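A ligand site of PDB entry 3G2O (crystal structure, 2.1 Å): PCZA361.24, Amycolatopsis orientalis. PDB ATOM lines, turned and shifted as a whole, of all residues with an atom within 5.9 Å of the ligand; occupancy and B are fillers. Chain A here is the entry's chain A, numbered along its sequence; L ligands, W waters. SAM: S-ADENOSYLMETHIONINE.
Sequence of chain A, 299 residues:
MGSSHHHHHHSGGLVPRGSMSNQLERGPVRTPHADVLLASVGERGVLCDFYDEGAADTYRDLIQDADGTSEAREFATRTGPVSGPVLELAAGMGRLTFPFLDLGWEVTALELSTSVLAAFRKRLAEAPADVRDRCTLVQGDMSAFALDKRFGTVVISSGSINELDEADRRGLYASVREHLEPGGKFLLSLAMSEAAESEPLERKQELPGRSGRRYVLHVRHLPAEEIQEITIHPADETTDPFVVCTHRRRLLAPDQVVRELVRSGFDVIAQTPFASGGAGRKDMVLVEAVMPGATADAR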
ATOM      1  N   GLU A  71     -30.604  12.847   7.367  1.00  0.00           N
ATOM      2  CA  GLU A  71     -29.564  12.744   8.391  1.00  0.00           C
ATOM      3  C   GLU A  71     -28.599  11.628   8.009  1.00  0.00           C
ATOM      4  O   GLU A  71     -27.380  11.801   8.069  1.00  0.00           O
ATOM      5  CB  GLU A  71     -30.163  12.517   9.794  1.00  0.00           C
ATOM      6  CG  GLU A  71     -29.096  12.451  10.901  1.00  0.00           C
ATOM      7  CD  GLU A  71     -29.648  12.209  12.302  1.00  0.00           C
ATOM      8  OE1 GLU A  71     -30.862  12.375  12.521  1.00  0.00           O
ATOM      9  OE2 GLU A  71     -28.842  11.867  13.199  1.00  0.00           O
ATOM     10  N   GLU A  88     -23.199   1.100  14.100  1.00  0.00           N
ATOM     11  CA  GLU A  88     -24.167   2.108  14.535  1.00  0.00           C
ATOM     12  C   GLU A  88     -24.663   1.881  15.966  1.00  0.00           C
ATOM     13  O   GLU A  88     -25.217   0.813  16.258  1.00  0.00           O
ATOM     14  CB  GLU A  88     -25.358   2.203  13.573  1.00  0.00           C
ATOM     15  CG  GLU A  88     -26.296   3.369  13.926  1.00  0.00           C
ATOM     16  CD  GLU A  88     -27.656   3.226  13.292  1.00  0.00           C
ATOM     17  OE1 GLU A  88     -27.837   2.322  12.458  1.00  0.00           O
ATOM     18  OE2 GLU A  88     -28.542   4.029  13.626  1.00  0.00           O
ATOM     19  N   LEU A  89     -24.473   2.888  16.826  1.00  0.00           N
ATOM     20  CA  LEU A  89     -24.770   2.773  18.270  1.00  0.00           C
ATOM     21  C   LEU A  89     -26.162   3.284  18.584  1.00  0.00           C
ATOM     22  O   LEU A  89     -26.564   4.320  18.064  1.00  0.00           O
ATOM     23  CB  LEU A  89     -23.755   3.574  19.139  1.00  0.00           C
ATOM     24  CG  LEU A  89     -22.291   3.153  18.957  1.00  0.00           C
ATOM     25  CD1 LEU A  89     -21.319   4.066  19.767  1.00  0.00           C
ATOM     26  CD2 LEU A  89     -22.072   1.679  19.335  1.00  0.00           C
ATOM     27  N   ALA A  90     -26.864   2.558  19.453  1.00  0.00           N
ATOM     28  CA  ALA A  90     -28.250   2.860  19.765  1.00  0.00           C
ATOM     29  C   ALA A  90     -29.070   2.996  18.468  1.00  0.00           C
ATOM     30  O   ALA A  90     -29.607   4.071  18.150  1.00  0.00           O
ATOM     31  CB  ALA A  90     -28.345   4.106  20.622  1.00  0.00           C
ATOM     32  N   ALA A  91     -29.165   1.897  17.712  1.00  0.00           N
ATOM     33  CA  ALA A  91     -29.784   1.912  16.373  1.00  0.00           C
ATOM     34  C   ALA A  91     -31.303   2.069  16.398  1.00  0.00           C
ATOM     35  O   ALA A  91     -31.914   2.495  15.397  1.00  0.00           O
ATOM     36  CB  ALA A  91     -29.378   0.668  15.590  1.00  0.00           C
ATOM     37  N   GLY A  92     -31.920   1.732  17.532  1.00  0.00           N
ATOM     38  CA  GLY A  92     -33.341   1.909  17.701  1.00  0.00           C
ATOM     39  C   GLY A  92     -34.050   0.899  16.832  1.00  0.00           C
ATOM     40  O   GLY A  92     -33.715  -0.297  16.850  1.00  0.00           O
ATOM     41  N   MET A  93     -35.022   1.366  16.068  1.00  0.00           N
ATOM     42  CA  MET A  93     -35.713   0.535  15.077  1.00  0.00           C
ATOM     43  C   MET A  93     -35.174   0.680  13.651  1.00  0.00           C
ATOM     44  O   MET A  93     -35.752   0.131  12.698  1.00  0.00           O
ATOM     45  CB  MET A  93     -37.217   0.803  15.107  1.00  0.00           C
ATOM     46  CG  MET A  93     -37.952  -0.175  15.984  1.00  0.00           C
ATOM     47  SD  MET A  93     -39.665   0.293  16.184  1.00  0.00           S
ATOM     48  CE  MET A  93     -40.129   0.790  14.509  1.00  0.00           C
ATOM     49  N   GLY A  94     -34.062   1.410  13.523  1.00  0.00           N
ATOM     50  CA  GLY A  94     -33.339   1.512  12.272  1.00  0.00           C
ATOM     51  C   GLY A  94     -33.782   2.657  11.387  1.00  0.00           C
ATOM     52  O   GLY A  94     -33.694   2.552  10.173  1.00  0.00           O
ATOM     53  N   ARG A  95     -34.234   3.747  11.996  1.00  0.00           N
ATOM     54  CA  ARG A  95     -34.542   5.001  11.280  1.00  0.00           C
ATOM     55  C   ARG A  95     -33.342   5.472  10.434  1.00  0.00           C
ATOM     56  O   ARG A  95     -33.519   6.069   9.376  1.00  0.00           O
ATOM     57  CB  ARG A  95     -34.986   6.095  12.268  1.00  0.00           C
ATOM     58  CG  ARG A  95     -35.224   7.478  11.666  1.00  0.00           C
ATOM     59  CD  ARG A  95     -35.552   8.567  12.689  1.00  0.00           C
ATOM     60  NE  ARG A  95     -34.369   8.991  13.446  1.00  0.00           N
ATOM     61  CZ  ARG A  95     -33.546   9.979  13.096  1.00  0.00           C
ATOM     62  NH1 ARG A  95     -33.767  10.709  12.010  1.00  0.00           N
ATOM     63  NH2 ARG A  95     -32.491  10.243  13.849  1.00  0.00           N
ATOM     64  N   LEU A  96     -32.130   5.194  10.893  1.00  0.00           N
ATOM     65  CA  LEU A  96     -30.931   5.480  10.119  1.00  0.00           C
ATOM     66  C   LEU A  96     -30.347   4.240   9.493  1.00  0.00           C
ATOM     67  O   LEU A  96     -29.798   4.295   8.406  1.00  0.00           O
ATOM     68  CB  LEU A  96     -29.848   6.142  11.001  1.00  0.00           C
ATOM     69  CG  LEU A  96     -30.027   7.561  11.535  1.00  0.00           C
ATOM     70  CD1 LEU A  96     -28.676   8.020  12.097  1.00  0.00           C
ATOM     71  CD2 LEU A  96     -30.526   8.532  10.467  1.00  0.00           C
ATOM     72  N   LEU A 110     -26.170  -1.820  17.178  1.00  0.00           N
ATOM     73  CA  LEU A 110     -26.184  -2.110  18.597  1.00  0.00           C
ATOM     74  C   LEU A 110     -27.343  -1.384  19.263  1.00  0.00           C
ATOM     75  O   LEU A 110     -27.578  -0.188  19.010  1.00  0.00           O
ATOM     76  CB  LEU A 110     -24.837  -1.724  19.222  1.00  0.00           C
ATOM     77  CG  LEU A 110     -24.735  -1.860  20.737  1.00  0.00           C
ATOM     78  CD1 LEU A 110     -23.349  -2.376  21.135  1.00  0.00           C
ATOM     79  CD2 LEU A 110     -25.052  -0.496  21.399  1.00  0.00           C
ATOM     80  N   GLU A 111     -28.046  -2.074  20.144  1.00  0.00           N
ATOM     81  CA  GLU A 111     -29.211  -1.501  20.778  1.00  0.00           C
ATOM     82  C   GLU A 111     -29.341  -2.162  22.148  1.00  0.00           C
ATOM     83  O   GLU A 111     -28.990  -3.344  22.268  1.00  0.00           O
ATOM     84  CB  GLU A 111     -30.445  -1.747  19.884  1.00  0.00           C
ATOM     85  CG  GLU A 111     -31.804  -1.456  20.487  1.00  0.00           C
ATOM     86  CD  GLU A 111     -31.942  -0.033  21.028  1.00  0.00           C
ATOM     87  OE1 GLU A 111     -31.601   0.943  20.327  1.00  0.00           O
ATOM     88  OE2 GLU A 111     -32.433   0.090  22.164  1.00  0.00           O
ATOM     89  N   LEU A 112     -29.816  -1.407  23.141  1.00  0.00           N
ATOM     90  CA  LEU A 112     -29.963  -1.882  24.532  1.00  0.00           C
ATOM     91  C   LEU A 112     -31.260  -2.628  24.792  1.00  0.00           C
ATOM     92  O   LEU A 112     -31.265  -3.641  25.512  1.00  0.00           O
ATOM     93  CB  LEU A 112     -29.860  -0.727  25.521  1.00  0.00           C
ATOM     94  CG  LEU A 112     -29.852  -1.010  27.041  1.00  0.00           C
ATOM     95  CD1 LEU A 112     -28.702  -1.911  27.472  1.00  0.00           C
ATOM     96  CD2 LEU A 112     -29.832   0.289  27.854  1.00  0.00           C
ATOM     97  N   SER A 113     -32.363  -2.107  24.247  1.00  0.00           N
ATOM     98  CA  SER A 113     -33.683  -2.649  24.551  1.00  0.00           C
ATOM     99  C   SER A 113     -34.010  -3.904  23.734  1.00  0.00           C
ATOM    100  O   SER A 113     -33.902  -3.927  22.494  1.00  0.00           O
ATOM    101  CB  SER A 113     -34.747  -1.582  24.351  1.00  0.00           C
ATOM    102  OG  SER A 113     -36.004  -2.204  24.205  1.00  0.00           O
ATOM    103  N   VAL A 116     -37.187  -3.326  21.521  1.00  0.00           N
ATOM    104  CA  VAL A 116     -36.784  -2.556  20.349  1.00  0.00           C
ATOM    105  C   VAL A 116     -36.040  -3.443  19.322  1.00  0.00           C
ATOM    106  O   VAL A 116     -36.304  -3.376  18.133  1.00  0.00           O
ATOM    107  CB  VAL A 116     -35.969  -1.287  20.728  1.00  0.00           C
ATOM    108  CG1 VAL A 116     -35.443  -0.580  19.493  1.00  0.00           C
ATOM    109  CG2 VAL A 116     -36.824  -0.312  21.559  1.00  0.00           C
ATOM    110  N   GLY A 140     -26.505  -4.492  23.397  1.00  0.00           N
ATOM    111  CA  GLY A 140     -25.406  -3.933  24.168  1.00  0.00           C
ATOM    112  C   GLY A 140     -25.665  -2.535  24.692  1.00  0.00           C
ATOM    113  O   GLY A 140     -26.576  -1.853  24.223  1.00  0.00           O
ATOM    114  N   ASP A 141     -24.875  -2.146  25.692  1.00  0.00           N
ATOM    115  CA  ASP A 141     -24.890  -0.810  26.274  1.00  0.00           C
ATOM    116  C   ASP A 141     -23.811   0.030  25.590  1.00  0.00           C
ATOM    117  O   ASP A 141     -22.649  -0.252  25.742  1.00  0.00           O
ATOM    118  CB  ASP A 141     -24.575  -0.909  27.773  1.00  0.00           C
ATOM    119  CG  ASP A 141     -24.855   0.372  28.526  1.00  0.00           C
ATOM    120  OD1 ASP A 141     -24.796   1.486  27.945  1.00  0.00           O
ATOM    121  OD2 ASP A 141     -25.116   0.273  29.723  1.00  0.00           O
ATOM    122  N   MET A 142     -24.200   1.064  24.835  1.00  0.00           N
ATOM    123  CA  MET A 142     -23.219   1.884  24.112  1.00  0.00           C
ATOM    124  C   MET A 142     -22.249   2.655  25.056  1.00  0.00           C
ATOM    125  O   MET A 142     -21.209   3.164  24.605  1.00  0.00           O
ATOM    126  CB  MET A 142     -23.944   2.855  23.199  1.00  0.00           C
ATOM    127  CG  MET A 142     -24.810   3.803  23.983  1.00  0.00           C
ATOM    128  SD  MET A 142     -25.590   5.069  22.989  1.00  0.00           S
ATOM    129  CE  MET A 142     -26.895   5.562  24.084  1.00  0.00           C
ATOM    130  N   SER A 143     -22.579   2.745  26.338  1.00  0.00           N
ATOM    131  CA  SER A 143     -21.663   3.345  27.333  1.00  0.00           C
ATOM    132  C   SER A 143     -20.610   2.347  27.868  1.00  0.00           C
ATOM    133  O   SER A 143     -19.639   2.736  28.520  1.00  0.00           O
ATOM    134  CB  SER A 143     -22.453   3.983  28.482  1.00  0.00           C
ATOM    135  OG  SER A 143     -22.884   3.035  29.464  1.00  0.00           O
ATOM    136  N   SER A 157     -26.417   8.988  16.654  1.00  0.00           N
ATOM    137  CA  SER A 157     -27.240  10.145  16.381  1.00  0.00           C
ATOM    138  C   SER A 157     -27.487  10.968  17.638  1.00  0.00           C
ATOM    139  O   SER A 157     -27.234  10.497  18.768  1.00  0.00           O
ATOM    140  CB  SER A 157     -28.563   9.730  15.724  1.00  0.00           C
ATOM    141  OG  SER A 157     -29.324   9.026  16.681  1.00  0.00           O
ATOM    142  N   SER A 158     -27.984  12.199  17.445  1.00  0.00           N
ATOM    143  CA  SER A 158     -28.181  13.128  18.536  1.00  0.00           C
ATOM    144  C   SER A 158     -29.051  12.551  19.649  1.00  0.00           C
ATOM    145  O   SER A 158     -28.717  12.675  20.845  1.00  0.00           O
ATOM    146  CB  SER A 158     -28.816  14.438  18.038  1.00  0.00           C
ATOM    147  OG  SER A 158     -28.978  15.346  19.113  1.00  0.00           O
ATOM    148  N   GLY A 159     -30.174  11.931  19.269  1.00  0.00           N
ATOM    149  CA  GLY A 159     -31.125  11.421  20.240  1.00  0.00           C
ATOM    150  C   GLY A 159     -30.474  10.438  21.201  1.00  0.00           C
ATOM    151  O   GLY A 159     -30.850  10.340  22.391  1.00  0.00           O
ATOM    152  N   SER A 160     -29.479   9.725  20.678  1.00  0.00           N
ATOM    153  CA  SER A 160     -28.835   8.638  21.386  1.00  0.00           C
ATOM    154  C   SER A 160     -27.789   9.134  22.385  1.00  0.00           C
ATOM    155  O   SER A 160     -27.851   8.774  23.540  1.00  0.00           O
ATOM    156  CB  SER A 160     -28.194   7.708  20.389  1.00  0.00           C
ATOM    157  OG  SER A 160     -29.149   7.247  19.465  1.00  0.00           O
ATOM    158  N   GLU A 163     -29.133  10.628  25.483  1.00  0.00           N
ATOM    159  CA  GLU A 163     -29.657   9.709  26.481  1.00  0.00           C
ATOM    160  C   GLU A 163     -28.678   9.519  27.645  1.00  0.00           C
ATOM    161  O   GLU A 163     -29.060   9.040  28.707  1.00  0.00           O
ATOM    162  CB  GLU A 163     -29.877   8.325  25.857  1.00  0.00           C
ATOM    163  CG  GLU A 163     -30.929   8.249  24.776  1.00  0.00           C
ATOM    164  CD  GLU A 163     -32.293   7.926  25.318  1.00  0.00           C
ATOM    165  OE1 GLU A 163     -32.523   6.763  25.743  1.00  0.00           O
ATOM    166  OE2 GLU A 163     -33.140   8.831  25.336  1.00  0.00           O
ATOM    167  N   LEU A 164     -27.417   9.890  27.450  1.00  0.00           N
ATOM    168  CA  LEU A 164     -26.333   9.503  28.387  1.00  0.00           C
ATOM    169  C   LEU A 164     -25.917  10.668  29.258  1.00  0.00           C
ATOM    170  O   LEU A 164     -25.738  11.789  28.757  1.00  0.00           O
ATOM    171  CB  LEU A 164     -25.139   9.008  27.576  1.00  0.00           C
ATOM    172  CG  LEU A 164     -25.304   7.727  26.743  1.00  0.00           C
ATOM    173  CD1 LEU A 164     -23.972   7.397  26.072  1.00  0.00           C
ATOM    174  CD2 LEU A 164     -25.797   6.577  27.638  1.00  0.00           C
ATOM    175  N   ARG A 249     -36.210  16.356  27.986  1.00  0.00           N
ATOM    176  CA  ARG A 249     -35.001  15.606  27.666  1.00  0.00           C
ATOM    177  C   ARG A 249     -33.726  16.462  27.624  1.00  0.00           C
ATOM    178  O   ARG A 249     -33.783  17.687  27.426  1.00  0.00           O
ATOM    179  CB  ARG A 249     -35.170  14.798  26.380  1.00  0.00           C
ATOM    180  CG  ARG A 249     -35.171  15.591  25.088  1.00  0.00           C
ATOM    181  CD  ARG A 249     -35.388  14.636  23.893  1.00  0.00           C
ATOM    182  NE  ARG A 249     -35.602  15.366  22.628  1.00  0.00           N
ATOM    183  CZ  ARG A 249     -35.894  14.805  21.454  1.00  0.00           C
ATOM    184  NH1 ARG A 249     -35.999  13.479  21.342  1.00  0.00           N
ATOM    185  NH2 ARG A 249     -36.070  15.569  20.372  1.00  0.00           N
HETATM  186  N   SAM L   1     -30.304   6.082  16.314  1.00  0.00           N
HETATM  187  CA  SAM L   1     -31.795   5.938  16.284  1.00  0.00           C
HETATM  188  C   SAM L   1     -32.427   7.026  15.421  1.00  0.00           C
HETATM  189  O   SAM L   1     -31.752   7.964  14.966  1.00  0.00           O
HETATM  190  OXT SAM L   1     -33.649   6.996  15.177  1.00  0.00           O
HETATM  191  CB  SAM L   1     -32.429   5.887  17.685  1.00  0.00           C
HETATM  192  CG  SAM L   1     -32.076   7.004  18.678  1.00  0.00           C
HETATM  193  SD  SAM L   1     -33.280   7.117  20.044  1.00  0.00           S
HETATM  194  CE  SAM L   1     -33.323   8.881  20.425  1.00  0.00           C
HETATM  195  C5' SAM L   1     -32.536   6.376  21.516  1.00  0.00           C
HETATM  196  C4' SAM L   1     -32.352   4.853  21.398  1.00  0.00           C
HETATM  197  O4' SAM L   1     -31.228   4.515  22.162  1.00  0.00           O
HETATM  198  C3' SAM L   1     -33.480   3.969  21.914  1.00  0.00           C
HETATM  199  O3' SAM L   1     -33.639   2.915  20.999  1.00  0.00           O
HETATM  200  C2' SAM L   1     -32.977   3.390  23.239  1.00  0.00           C
HETATM  201  O2' SAM L   1     -33.461   2.085  23.533  1.00  0.00           O
HETATM  202  C1' SAM L   1     -31.489   3.355  22.915  1.00  0.00           C
HETATM  203  N9  SAM L   1     -30.598   3.390  24.068  1.00  0.00           N
HETATM  204  C8  SAM L   1     -30.749   4.095  25.227  1.00  0.00           C
HETATM  205  N7  SAM L   1     -29.667   3.848  26.008  1.00  0.00           N
HETATM  206  C5  SAM L   1     -28.852   3.000  25.349  1.00  0.00           C
HETATM  207  C6  SAM L   1     -27.631   2.438  25.705  1.00  0.00           C
HETATM  208  N6  SAM L   1     -27.071   2.721  26.898  1.00  0.00           N
HETATM  209  N1  SAM L   1     -27.033   1.593  24.781  1.00  0.00           N
HETATM  210  C2  SAM L   1     -27.604   1.293  23.550  1.00  0.00           C
HETATM  211  N3  SAM L   1     -28.825   1.853  23.208  1.00  0.00           N
HETATM  212  C4  SAM L   1     -29.428   2.697  24.110  1.00  0.00           C
HETATM  213  O   HOH W   1     -27.720   6.381  17.213  1.00  0.00           O
HETATM  214  O   HOH W   2     -33.845  10.090  17.682  1.00  0.00           O
HETATM  215  O   HOH W   3     -36.227   3.453  19.788  1.00  0.00           O
HETATM  216  O   HOH W   4     -34.822   4.574  15.394  1.00  0.00           O
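OE2 of Glu 111 sits at hydrogen-bond distance from O2' of the ligand (2.6 Å). The backbone NH (N) of Leu 112 lies within hydrogen-bond range of a nitrogen (N3) of the ligand, 3.4 Å away. N1 of the ligand sits at hydrogen-bond distance from N of Met 142. A nitrogen (N) of the ligand is in hydrogen-bond range of the backbone carbonyl oxygen (O) of Ala 90, 2.8 Å away. NH2 of Arg 95 is in salt-bridge range of O of the ligand (2.6 Å). The side-chain hydroxyl (OG) of Ser 157 is in hydrogen-bond range of a nitrogen (N) of the ligand (3.1 Å). A nitrogen (N6) of the ligand is in hydrogen-bond range of the side-chain carboxylate (OD1) of Asp 141 (2.8 Å). OE2 of Glu 88 lies within salt-bridge range of N of the ligand (3.8 Å).
OD1 of Asp 141 is in hydrogen-bond range of OG of Ser 143 (2.9 Å). N of Ala 91 sits at hydrogen-bond distance from O of Leu 110, at 2.9 Å. N of Gly 140 sits at hydrogen-bond distance from O of Glu 111, 3.0 Å away. The side-chain carboxylate (OE2) of Glu 111 is in hydrogen-bond range of the backbone NH (N) of Ser 113 (3.0 Å). The backbone carbonyl oxygen of Leu 110 lies within hydrogen-bond range of the backbone NH of Ala 90, at 2.9 Å. NH2 of Arg 95 lies within salt-bridge range of OE1 of Glu 71 (3.0 Å). N of Val 116 sits at hydrogen-bond distance from OG of Ser 113, at 3.1 Å. The side-chain carboxylate of Glu 111 lies within hydrogen-bond range of the backbone NH of Gly 92 (2.9 Å).
Residues that only touch the ligand: Ser 160, Glu 163, Gly 159, Gly 140, Gly 92, Ala 91, Leu 110, Leu 96 and Ser 113. Hydrophobic or aromatic side chains that line the ligand: Ala 90, Leu 96, Leu 110, Leu 112 and Met 142. Of the 26 residues printed, 17 come within 4 Å of the ligand. The nearest printed residue that does not touch the ligand is Leu 164 (4.1 Å).
Water W4 lies within hydrogen-bond range of OXT of the ligand (2.7 Å) and N of Met 93 (3.3 Å). Water W1 lies within hydrogen-bond range of O of Leu 89, N of the ligand, OG of Ser 160, N of Ser 157 and O of Ala 90.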
